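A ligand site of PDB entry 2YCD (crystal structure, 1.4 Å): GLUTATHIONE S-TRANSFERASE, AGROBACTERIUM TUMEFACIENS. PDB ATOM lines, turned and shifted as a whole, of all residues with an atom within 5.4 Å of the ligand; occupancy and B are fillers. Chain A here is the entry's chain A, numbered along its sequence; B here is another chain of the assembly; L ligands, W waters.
OE2 of Glu 85 is in hydrogen-bond range of OG1 of Thr 121 of chain B. The side-chain amide nitrogen of Gln 72 sits close to the guanidinium group of Arg 156 of chain B (3.3 Å). OE1 of Gln 68 sits at hydrogen-bond distance from N of Gln 72, at 3.2 Å. ND2 of Asn 120 of chain B lies close to NH1 of Arg 34 (3.5 Å). The side-chain carboxylate of Asp 27 lies within hydrogen-bond range of the backbone NH of Leu 32 (2.8 Å). OD2 of Asp 27 sits at hydrogen-bond distance from N of Ala 33 (3.5 Å). The backbone carbonyl oxygen of Asp 27 sits at hydrogen-bond distance from the guanidinium group of Arg 30 (2.8 Å).
O of Pro 26 lies close to O8 of the ligand (3.1 Å). Merely in contact with the ligand: Phe 22 (3.7 Å), Leu 32 (3.4 Å), Ala 33 (3.8 Å), Met 59 (3.5 Å), Pro 74 (3.8 Å) and Arg 187 (3.5 Å). 15 residues have an atom within 4 Å of the ligand: Phe 22, Pro 26, Asp 27, Leu 32, Ala 33, Arg 34, Met 59, Gln 72, Ile 73, Pro 74, Glu 85, Ser 86, Arg 187, Asn 120 of chain B and Thr 121 of chain B.
Water W5 lies within hydrogen-bond range of O5 of the ligand (2.7 Å) and NH2 of Arg 156 of chain B (3.0 Å). Water W1 lies within hydrogen-bond range of the backbone carbonyl oxygen of Pro 74 (2.7 Å), an oxygen (O2) of the ligand (2.7 Å), the backbone NH of Glu 85 (2.9 Å) and the side-chain amide nitrogen of Gln 68 (2.9 Å). Water W4 lies within hydrogen-bond range of the backbone carbonyl oxygen (O) of Pro 26 (2.6 Å), the guanidinium group (NH2) of Arg 30 (2.9 Å) and an oxygen (O8) of the ligand (3.2 Å). Water W6 lies within hydrogen-bond range of OE1 of Glu 85 (2.8 Å), N of Gly 87 (3.0 Å), ND2 of Asn 120 of chain B (3.0 Å) and O1 of the ligand (3.2 Å). Water W2 bridges NH1 of Arg 156 of chain B (3.1 Å) and O5 of the ligand (3.3 Å).
The side-chain carboxylate (OE1) of Glu 85 lies within salt-bridge range of a nitrogen (N1) of the ligand (2.7 Å). N of Ser 86 sits at hydrogen-bond distance from O2 of the ligand. OG of Ser 86 sits at hydrogen-bond distance from O1 of the ligand, at 2.7 Å. An oxygen (O4) of the ligand lies within hydrogen-bond range of the backbone NH (N) of Ile 73 (2.9 Å). The backbone carbonyl oxygen (O) of Ile 73 is in hydrogen-bond range of a nitrogen (N2) of the ligand (2.8 Å). O5 of the ligand is in hydrogen-bond range of NE2 of Gln 72 (2.9 Å). The side-chain hydroxyl of Thr 121 of chain B is in hydrogen-bond range of a nitrogen (N1) of the ligand, at 2.9 Å. N1 of the ligand is in hydrogen-bond range of O of Asn 120 of chain B, at 3.1 Å. A nitrogen (N1) of the ligand sits close to the side-chain amide nitrogen of Asn 120 of chain B (3.0 Å). The backbone NH (N) of Asp 27 sits close to an oxygen (O8) of the ligand, 3.4 Å away. The backbone NH (N) of Arg 34 lies close to a sulfur (S1) of the ligand (3.5 Å). NH1 of Arg 34 lies within salt-bridge range of O1 of the ligand, 3.4 Å away.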
ATOM      1  N   PHE A  22      26.567  -1.199 -14.175  1.00  0.00           N
ATOM      2  CA  PHE A  22      26.390  -0.455 -15.427  1.00  0.00           C
ATOM      3  C   PHE A  22      27.096   0.899 -15.342  1.00  0.00           C
ATOM      4  O   PHE A  22      26.968   1.608 -14.343  1.00  0.00           O
ATOM      5  CB  PHE A  22      24.903  -0.150 -15.700  1.00  0.00           C
ATOM      6  CG  PHE A  22      24.055  -1.343 -16.098  1.00  0.00           C
ATOM      7  CD1 PHE A  22      24.176  -1.917 -17.356  1.00  0.00           C
ATOM      8  CD2 PHE A  22      23.070  -1.804 -15.245  1.00  0.00           C
ATOM      9  CE1 PHE A  22      23.369  -2.977 -17.736  1.00  0.00           C
ATOM     10  CE2 PHE A  22      22.253  -2.874 -15.606  1.00  0.00           C
ATOM     11  CZ  PHE A  22      22.394  -3.453 -16.855  1.00  0.00           C
ATOM     12  N   PRO A  26      20.094   1.459 -16.959  1.00  0.00           N
ATOM     13  CA  PRO A  26      18.785   1.717 -17.575  1.00  0.00           C
ATOM     14  C   PRO A  26      17.695   1.997 -16.539  1.00  0.00           C
ATOM     15  O   PRO A  26      16.533   2.163 -16.906  1.00  0.00           O
ATOM     16  CB  PRO A  26      18.495   0.419 -18.340  1.00  0.00           C
ATOM     17  CG  PRO A  26      19.277  -0.637 -17.606  1.00  0.00           C
ATOM     18  CD  PRO A  26      20.516   0.060 -17.103  1.00  0.00           C
ATOM     19  N   ASP A  27      18.051   2.077 -15.258  1.00  0.00           N
ATOM     20  CA  ASP A  27      17.055   2.263 -14.207  1.00  0.00           C
ATOM     21  C   ASP A  27      16.779   3.725 -13.806  1.00  0.00           C
ATOM     22  O   ASP A  27      15.996   3.974 -12.883  1.00  0.00           O
ATOM     23  CB  ASP A  27      17.379   1.419 -12.971  1.00  0.00           C
ATOM     24  CG  ASP A  27      18.550   1.959 -12.154  1.00  0.00           C
ATOM     25  OD1 ASP A  27      19.217   2.910 -12.592  1.00  0.00           O
ATOM     26  OD2 ASP A  27      18.790   1.407 -11.070  1.00  0.00           O
ATOM     27  N   ARG A  30      17.406   4.819 -10.055  1.00  0.00           N
ATOM     28  CA  ARG A  30      16.461   4.410  -9.021  1.00  0.00           C
ATOM     29  C   ARG A  30      16.929   3.213  -8.191  1.00  0.00           C
ATOM     30  O   ARG A  30      16.192   2.761  -7.326  1.00  0.00           O
ATOM     31  CB  ARG A  30      15.085   4.105  -9.629  1.00  0.00           C
ATOM     32  CG  ARG A  30      14.407   5.343 -10.262  1.00  0.00           C
ATOM     33  CD  ARG A  30      13.098   4.982 -10.954  1.00  0.00           C
ATOM     34  NE  ARG A  30      13.298   4.088 -12.093  1.00  0.00           N
ATOM     35  CZ  ARG A  30      12.387   3.222 -12.529  1.00  0.00           C
ATOM     36  NH1 ARG A  30      11.192   3.157 -11.945  1.00  0.00           N
ATOM     37  NH2 ARG A  30      12.661   2.434 -13.564  1.00  0.00           N
ATOM     38  N   LEU A  32      17.505  -0.009  -9.020  1.00  0.00           N
ATOM     39  CA  LEU A  32      16.726  -1.217  -9.241  1.00  0.00           C
ATOM     40  C   LEU A  32      17.544  -2.321  -9.887  1.00  0.00           C
ATOM     41  O   LEU A  32      17.090  -3.467  -9.918  1.00  0.00           O
ATOM     42  CB  LEU A  32      15.488  -0.916 -10.089  1.00  0.00           C
ATOM     43  CG  LEU A  32      14.494   0.089  -9.514  1.00  0.00           C
ATOM     44  CD1 LEU A  32      13.439   0.449 -10.573  1.00  0.00           C
ATOM     45  CD2 LEU A  32      13.839  -0.439  -8.248  1.00  0.00           C
ATOM     46  N   ALA A  33      18.722  -2.014 -10.399  1.00  0.00           N
ATOM     47  CA  ALA A  33      19.596  -3.035 -10.974  1.00  0.00           C
ATOM     48  C   ALA A  33      20.181  -3.929  -9.873  1.00  0.00           C
ATOM     49  O   ALA A  33      20.200  -3.540  -8.690  1.00  0.00           O
ATOM     50  CB  ALA A  33      20.683  -2.409 -11.836  1.00  0.00           C
ATOM     51  N   ARG A  34      20.674  -5.098 -10.259  1.00  0.00           N
ATOM     52  CA  ARG A  34      21.018  -6.142  -9.284  1.00  0.00           C
ATOM     53  C   ARG A  34      22.324  -5.932  -8.528  1.00  0.00           C
ATOM     54  O   ARG A  34      22.653  -6.716  -7.636  1.00  0.00           O
ATOM     55  CB  ARG A  34      20.958  -7.534  -9.920  1.00  0.00           C
ATOM     56  CG  ARG A  34      19.539  -7.926 -10.333  1.00  0.00           C
ATOM     57  CD  ARG A  34      19.544  -9.236 -11.090  1.00  0.00           C
ATOM     58  NE  ARG A  34      18.223  -9.592 -11.626  1.00  0.00           N
ATOM     59  CZ  ARG A  34      17.356 -10.399 -11.009  1.00  0.00           C
ATOM     60  NH1 ARG A  34      17.647 -10.912  -9.822  1.00  0.00           N
ATOM     61  NH2 ARG A  34      16.194 -10.672 -11.584  1.00  0.00           N
ATOM     62  N   MET A  59      30.174  -5.131 -21.690  1.00  0.00           N
ATOM     63  CA  MET A  59      29.542  -6.271 -21.032  1.00  0.00           C
ATOM     64  C   MET A  59      29.412  -7.469 -21.963  1.00  0.00           C
ATOM     65  O   MET A  59      29.276  -8.606 -21.511  1.00  0.00           O
ATOM     66  CB  MET A  59      28.163  -5.878 -20.507  1.00  0.00           C
ATOM     67  CG  MET A  59      28.243  -4.899 -19.374  1.00  0.00           C
ATOM     68  SD  MET A  59      26.612  -4.408 -18.800  1.00  0.00           S
ATOM     69  CE  MET A  59      25.866  -5.988 -18.561  1.00  0.00           C
ATOM     70  N   GLN A  68      31.495 -13.059 -15.506  1.00  0.00           N
ATOM     71  CA  GLN A  68      30.077 -13.357 -15.496  1.00  0.00           C
ATOM     72  C   GLN A  68      29.770 -14.082 -16.806  1.00  0.00           C
ATOM     73  O   GLN A  68      29.787 -13.474 -17.873  1.00  0.00           O
ATOM     74  CB  GLN A  68      29.273 -12.066 -15.323  1.00  0.00           C
ATOM     75  CG  GLN A  68      28.041 -12.183 -14.419  1.00  0.00           C
ATOM     76  CD  GLN A  68      26.874 -12.852 -15.105  1.00  0.00           C
ATOM     77  OE1 GLN A  68      26.938 -13.196 -16.290  1.00  0.00           O
ATOM     78  NE2 GLN A  68      25.776 -13.016 -14.377  1.00  0.00           N
ATOM     79  N   GLY A  71      27.306 -12.665 -19.385  1.00  0.00           N
ATOM     80  CA  GLY A  71      27.494 -11.292 -19.837  1.00  0.00           C
ATOM     81  C   GLY A  71      26.630 -10.269 -19.126  1.00  0.00           C
ATOM     82  O   GLY A  71      26.234  -9.260 -19.724  1.00  0.00           O
ATOM     83  N   GLN A  72      26.339 -10.526 -17.852  1.00  0.00           N
ATOM     84  CA  GLN A  72      25.474  -9.654 -17.077  1.00  0.00           C
ATOM     85  C   GLN A  72      26.218  -9.092 -15.867  1.00  0.00           C
ATOM     86  O   GLN A  72      27.344  -9.510 -15.570  1.00  0.00           O
ATOM     87  CB  GLN A  72      24.217 -10.410 -16.631  1.00  0.00           C
ATOM     88  CG  GLN A  72      23.326 -10.801 -17.804  1.00  0.00           C
ATOM     89  CD  GLN A  72      21.946 -11.208 -17.394  1.00  0.00           C
ATOM     90  OE1 GLN A  72      21.765 -12.176 -16.643  1.00  0.00           O
ATOM     91  NE2 GLN A  72      20.939 -10.492 -17.898  1.00  0.00           N
ATOM     92  N   ILE A  73      25.584  -8.157 -15.169  1.00  0.00           N
ATOM     93  CA  ILE A  73      26.109  -7.672 -13.881  1.00  0.00           C
ATOM     94  C   ILE A  73      25.103  -8.036 -12.771  1.00  0.00           C
ATOM     95  O   ILE A  73      23.914  -8.225 -13.047  1.00  0.00           O
ATOM     96  CB  ILE A  73      26.421  -6.139 -13.912  1.00  0.00           C
ATOM     97  CG1 ILE A  73      25.162  -5.280 -14.143  1.00  0.00           C
ATOM     98  CG2 ILE A  73      27.444  -5.823 -14.997  1.00  0.00           C
ATOM     99  CD1 ILE A  73      24.432  -4.890 -12.851  1.00  0.00           C
ATOM    100  N   PRO A  74      25.550  -8.147 -11.514  1.00  0.00           N
ATOM    101  CA  PRO A  74      26.912  -7.917 -11.023  1.00  0.00           C
ATOM    102  C   PRO A  74      27.784  -9.163 -10.920  1.00  0.00           C
ATOM    103  O   PRO A  74      27.300 -10.290 -10.802  1.00  0.00           O
ATOM    104  CB  PRO A  74      26.658  -7.396  -9.605  1.00  0.00           C
ATOM    105  CG  PRO A  74      25.423  -8.156  -9.164  1.00  0.00           C
ATOM    106  CD  PRO A  74      24.584  -8.333 -10.411  1.00  0.00           C
ATOM    107  N   PHE A  84      29.596 -14.734  -9.196  1.00  0.00           N
ATOM    108  CA  PHE A  84      28.479 -14.079  -9.854  1.00  0.00           C
ATOM    109  C   PHE A  84      27.197 -14.569  -9.177  1.00  0.00           C
ATOM    110  O   PHE A  84      27.257 -15.411  -8.268  1.00  0.00           O
ATOM    111  CB  PHE A  84      28.518 -14.264 -11.382  1.00  0.00           C
ATOM    112  CG  PHE A  84      28.152 -15.634 -11.840  1.00  0.00           C
ATOM    113  CD1 PHE A  84      29.043 -16.682 -11.709  1.00  0.00           C
ATOM    114  CD2 PHE A  84      26.908 -15.880 -12.407  1.00  0.00           C
ATOM    115  CE1 PHE A  84      28.708 -17.967 -12.156  1.00  0.00           C
ATOM    116  CE2 PHE A  84      26.560 -17.162 -12.855  1.00  0.00           C
ATOM    117  CZ  PHE A  84      27.456 -18.214 -12.702  1.00  0.00           C
ATOM    118  N   GLU A  85      26.067 -14.029  -9.633  1.00  0.00           N
ATOM    119  CA  GLU A  85      24.729 -14.210  -9.032  1.00  0.00           C
ATOM    120  C   GLU A  85      24.541 -13.329  -7.814  1.00  0.00           C
ATOM    121  O   GLU A  85      25.140 -13.590  -6.778  1.00  0.00           O
ATOM    122  CB  GLU A  85      24.396 -15.662  -8.695  1.00  0.00           C
ATOM    123  CG  GLU A  85      24.241 -16.560  -9.942  1.00  0.00           C
ATOM    124  CD  GLU A  85      23.089 -16.149 -10.827  1.00  0.00           C
ATOM    125  OE1 GLU A  85      22.065 -15.632 -10.332  1.00  0.00           O
ATOM    126  OE2 GLU A  85      23.190 -16.372 -12.060  1.00  0.00           O
ATOM    127  N   SER A  86      23.738 -12.279  -7.951  1.00  0.00           N
ATOM    128  CA  SER A  86      23.453 -11.385  -6.835  1.00  0.00           C
ATOM    129  C   SER A  86      23.053 -12.133  -5.564  1.00  0.00           C
ATOM    130  O   SER A  86      23.528 -11.788  -4.474  1.00  0.00           O
ATOM    131  CB  SER A  86      22.390 -10.361  -7.244  1.00  0.00           C
ATOM    132  OG  SER A  86      21.160 -10.979  -7.560  1.00  0.00           O
ATOM    133  N   GLY A  87      22.241 -13.192  -5.688  1.00  0.00           N
ATOM    134  CA  GLY A  87      21.845 -13.960  -4.504  1.00  0.00           C
ATOM    135  C   GLY A  87      23.034 -14.642  -3.835  1.00  0.00           C
ATOM    136  O   GLY A  87      23.134 -14.689  -2.593  1.00  0.00           O
ATOM    137  N   ARG A 187      10.869  -3.357  -7.527  1.00  0.00           N
ATOM    138  CA  ARG A 187      10.541  -3.332  -8.958  1.00  0.00           C
ATOM    139  C   ARG A 187       9.078  -3.012  -9.220  1.00  0.00           C
ATOM    140  O   ARG A 187       8.698  -2.683 -10.348  1.00  0.00           O
ATOM    141  CB  ARG A 187      10.955  -4.634  -9.636  1.00  0.00           C
ATOM    142  CG  ARG A 187      12.446  -4.849  -9.525  1.00  0.00           C
ATOM    143  CD  ARG A 187      12.914  -6.062 -10.275  1.00  0.00           C
ATOM    144  NE  ARG A 187      12.980  -5.801 -11.707  1.00  0.00           N
ATOM    145  CZ  ARG A 187      13.875  -6.355 -12.519  1.00  0.00           C
ATOM    146  NH1 ARG A 187      14.781  -7.210 -12.053  1.00  0.00           N
ATOM    147  NH2 ARG A 187      13.839  -6.069 -13.809  1.00  0.00           N
ATOM    148  N   ASN B 120      18.168 -18.935 -11.030  1.00  0.00           N
ATOM    149  CA  ASN B 120      17.888 -17.513 -11.233  1.00  0.00           C
ATOM    150  C   ASN B 120      18.411 -16.949 -12.566  1.00  0.00           C
ATOM    151  O   ASN B 120      18.163 -15.788 -12.885  1.00  0.00           O
ATOM    152  CB  ASN B 120      18.423 -16.689 -10.040  1.00  0.00           C
ATOM    153  CG  ASN B 120      17.747 -15.320  -9.882  1.00  0.00           C
ATOM    154  OD1 ASN B 120      16.519 -15.217  -9.870  1.00  0.00           O
ATOM    155  ND2 ASN B 120      18.542 -14.292  -9.727  1.00  0.00           N
ATOM    156  N   THR B 121      19.171 -17.762 -13.304  1.00  0.00           N
ATOM    157  CA  THR B 121      19.601 -17.393 -14.645  1.00  0.00           C
ATOM    158  C   THR B 121      19.124 -18.423 -15.681  1.00  0.00           C
ATOM    159  O   THR B 121      18.440 -18.067 -16.673  1.00  0.00           O
ATOM    160  CB  THR B 121      21.125 -17.161 -14.708  1.00  0.00           C
ATOM    161  OG1 THR B 121      21.442 -15.995 -13.924  1.00  0.00           O
ATOM    162  CG2 THR B 121      21.604 -16.935 -16.143  1.00  0.00           C
ATOM    163  N   ARG B 156      21.261 -18.294 -23.840  1.00  0.00           N
ATOM    164  CA  ARG B 156      21.699 -18.751 -22.519  1.00  0.00           C
ATOM    165  C   ARG B 156      22.335 -20.135 -22.568  1.00  0.00           C
ATOM    166  O   ARG B 156      23.308 -20.396 -21.851  1.00  0.00           O
ATOM    167  CB  ARG B 156      20.535 -18.758 -21.532  1.00  0.00           C
ATOM    168  CG  ARG B 156      20.075 -17.371 -21.136  1.00  0.00           C
ATOM    169  CD  ARG B 156      21.049 -16.684 -20.168  1.00  0.00           C
ATOM    170  NE  ARG B 156      20.550 -15.365 -19.825  1.00  0.00           N
ATOM    171  CZ  ARG B 156      21.062 -14.219 -20.238  1.00  0.00           C
ATOM    172  NH1 ARG B 156      22.140 -14.190 -21.003  1.00  0.00           N
ATOM    173  NH2 ARG B 156      20.498 -13.076 -19.855  1.00  0.00           N
HETATM  174  N1  LIG L   1      20.585 -14.039 -11.913  1.00  0.00           N
HETATM  175  C1  LIG L   1      21.455 -12.870 -12.123  1.00  0.00           C
HETATM  176  C2  LIG L   1      21.749 -12.205 -10.805  1.00  0.00           C
HETATM  177  O1  LIG L   1      20.821 -12.151  -9.967  1.00  0.00           O
HETATM  178  O2  LIG L   1      22.889 -11.708 -10.610  1.00  0.00           O
HETATM  179  C3  LIG L   1      20.755 -11.934 -13.117  1.00  0.00           C
HETATM  180  C4  LIG L   1      21.668 -10.764 -13.493  1.00  0.00           C
HETATM  181  C5  LIG L   1      20.968  -9.757 -14.388  1.00  0.00           C
HETATM  182  O3  LIG L   1      19.804  -9.963 -14.742  1.00  0.00           O
HETATM  183  N2  LIG L   1      21.669  -8.681 -14.724  1.00  0.00           N
HETATM  184  C6  LIG L   1      21.114  -7.620 -15.562  1.00  0.00           C
HETATM  185  C7  LIG L   1      22.006  -7.298 -16.724  1.00  0.00           C
HETATM  186  O4  LIG L   1      23.233  -7.332 -16.622  1.00  0.00           O
HETATM  187  C8  LIG L   1      21.061  -6.308 -14.738  1.00  0.00           C
HETATM  188  S1  LIG L   1      19.922  -6.332 -13.394  1.00  0.00           S
HETATM  189  N3  LIG L   1      21.386  -6.969 -17.855  1.00  0.00           N
HETATM  190  C9  LIG L   1      22.062  -6.563 -19.081  1.00  0.00           C
HETATM  191  C10 LIG L   1      21.979  -7.576 -20.183  1.00  0.00           C
HETATM  192  O5  LIG L   1      21.283  -8.600 -20.034  1.00  0.00           O
HETATM  193  O6  LIG L   1      22.642  -7.324 -21.218  1.00  0.00           O
HETATM  194  C11 LIG L   1      18.305  -6.419 -14.112  1.00  0.00           C
HETATM  195  C12 LIG L   1      17.666  -5.053 -14.250  1.00  0.00           C
HETATM  196  C13 LIG L   1      17.778  -4.358 -15.434  1.00  0.00           C
HETATM  197  C14 LIG L   1      17.178  -3.106 -15.559  1.00  0.00           C
HETATM  198  C15 LIG L   1      16.469  -2.569 -14.493  1.00  0.00           C
HETATM  199  N4  LIG L   1      15.850  -1.311 -14.626  1.00  0.00           N
HETATM  200  O7  LIG L   1      15.128  -0.865 -13.735  1.00  0.00           O
HETATM  201  O8  LIG L   1      16.030  -0.671 -15.644  1.00  0.00           O
HETATM  202  C16 LIG L   1      16.353  -3.284 -13.311  1.00  0.00           C
HETATM  203  C17 LIG L   1      16.953  -4.537 -13.187  1.00  0.00           C
HETATM  204  O   HOH W   1      25.383 -12.016 -11.648  1.00  0.00           O
HETATM  205  O   HOH W   2      22.835 -11.199 -21.251  1.00  0.00           O
HETATM  206  O   HOH W   3      17.668 -11.955 -14.880  1.00  0.00           O
HETATM  207  O   HOH W   4      14.069   1.778 -16.055  1.00  0.00           O
HETATM  208  O   HOH W   5      19.693 -10.471 -21.189  1.00  0.00           O
HETATM  209  O   HOH W   6      20.976 -14.650  -7.940  1.00  0.00           O
HETATM  210  O   HOH W   7      18.189  -7.624 -17.835  1.00  0.00           O
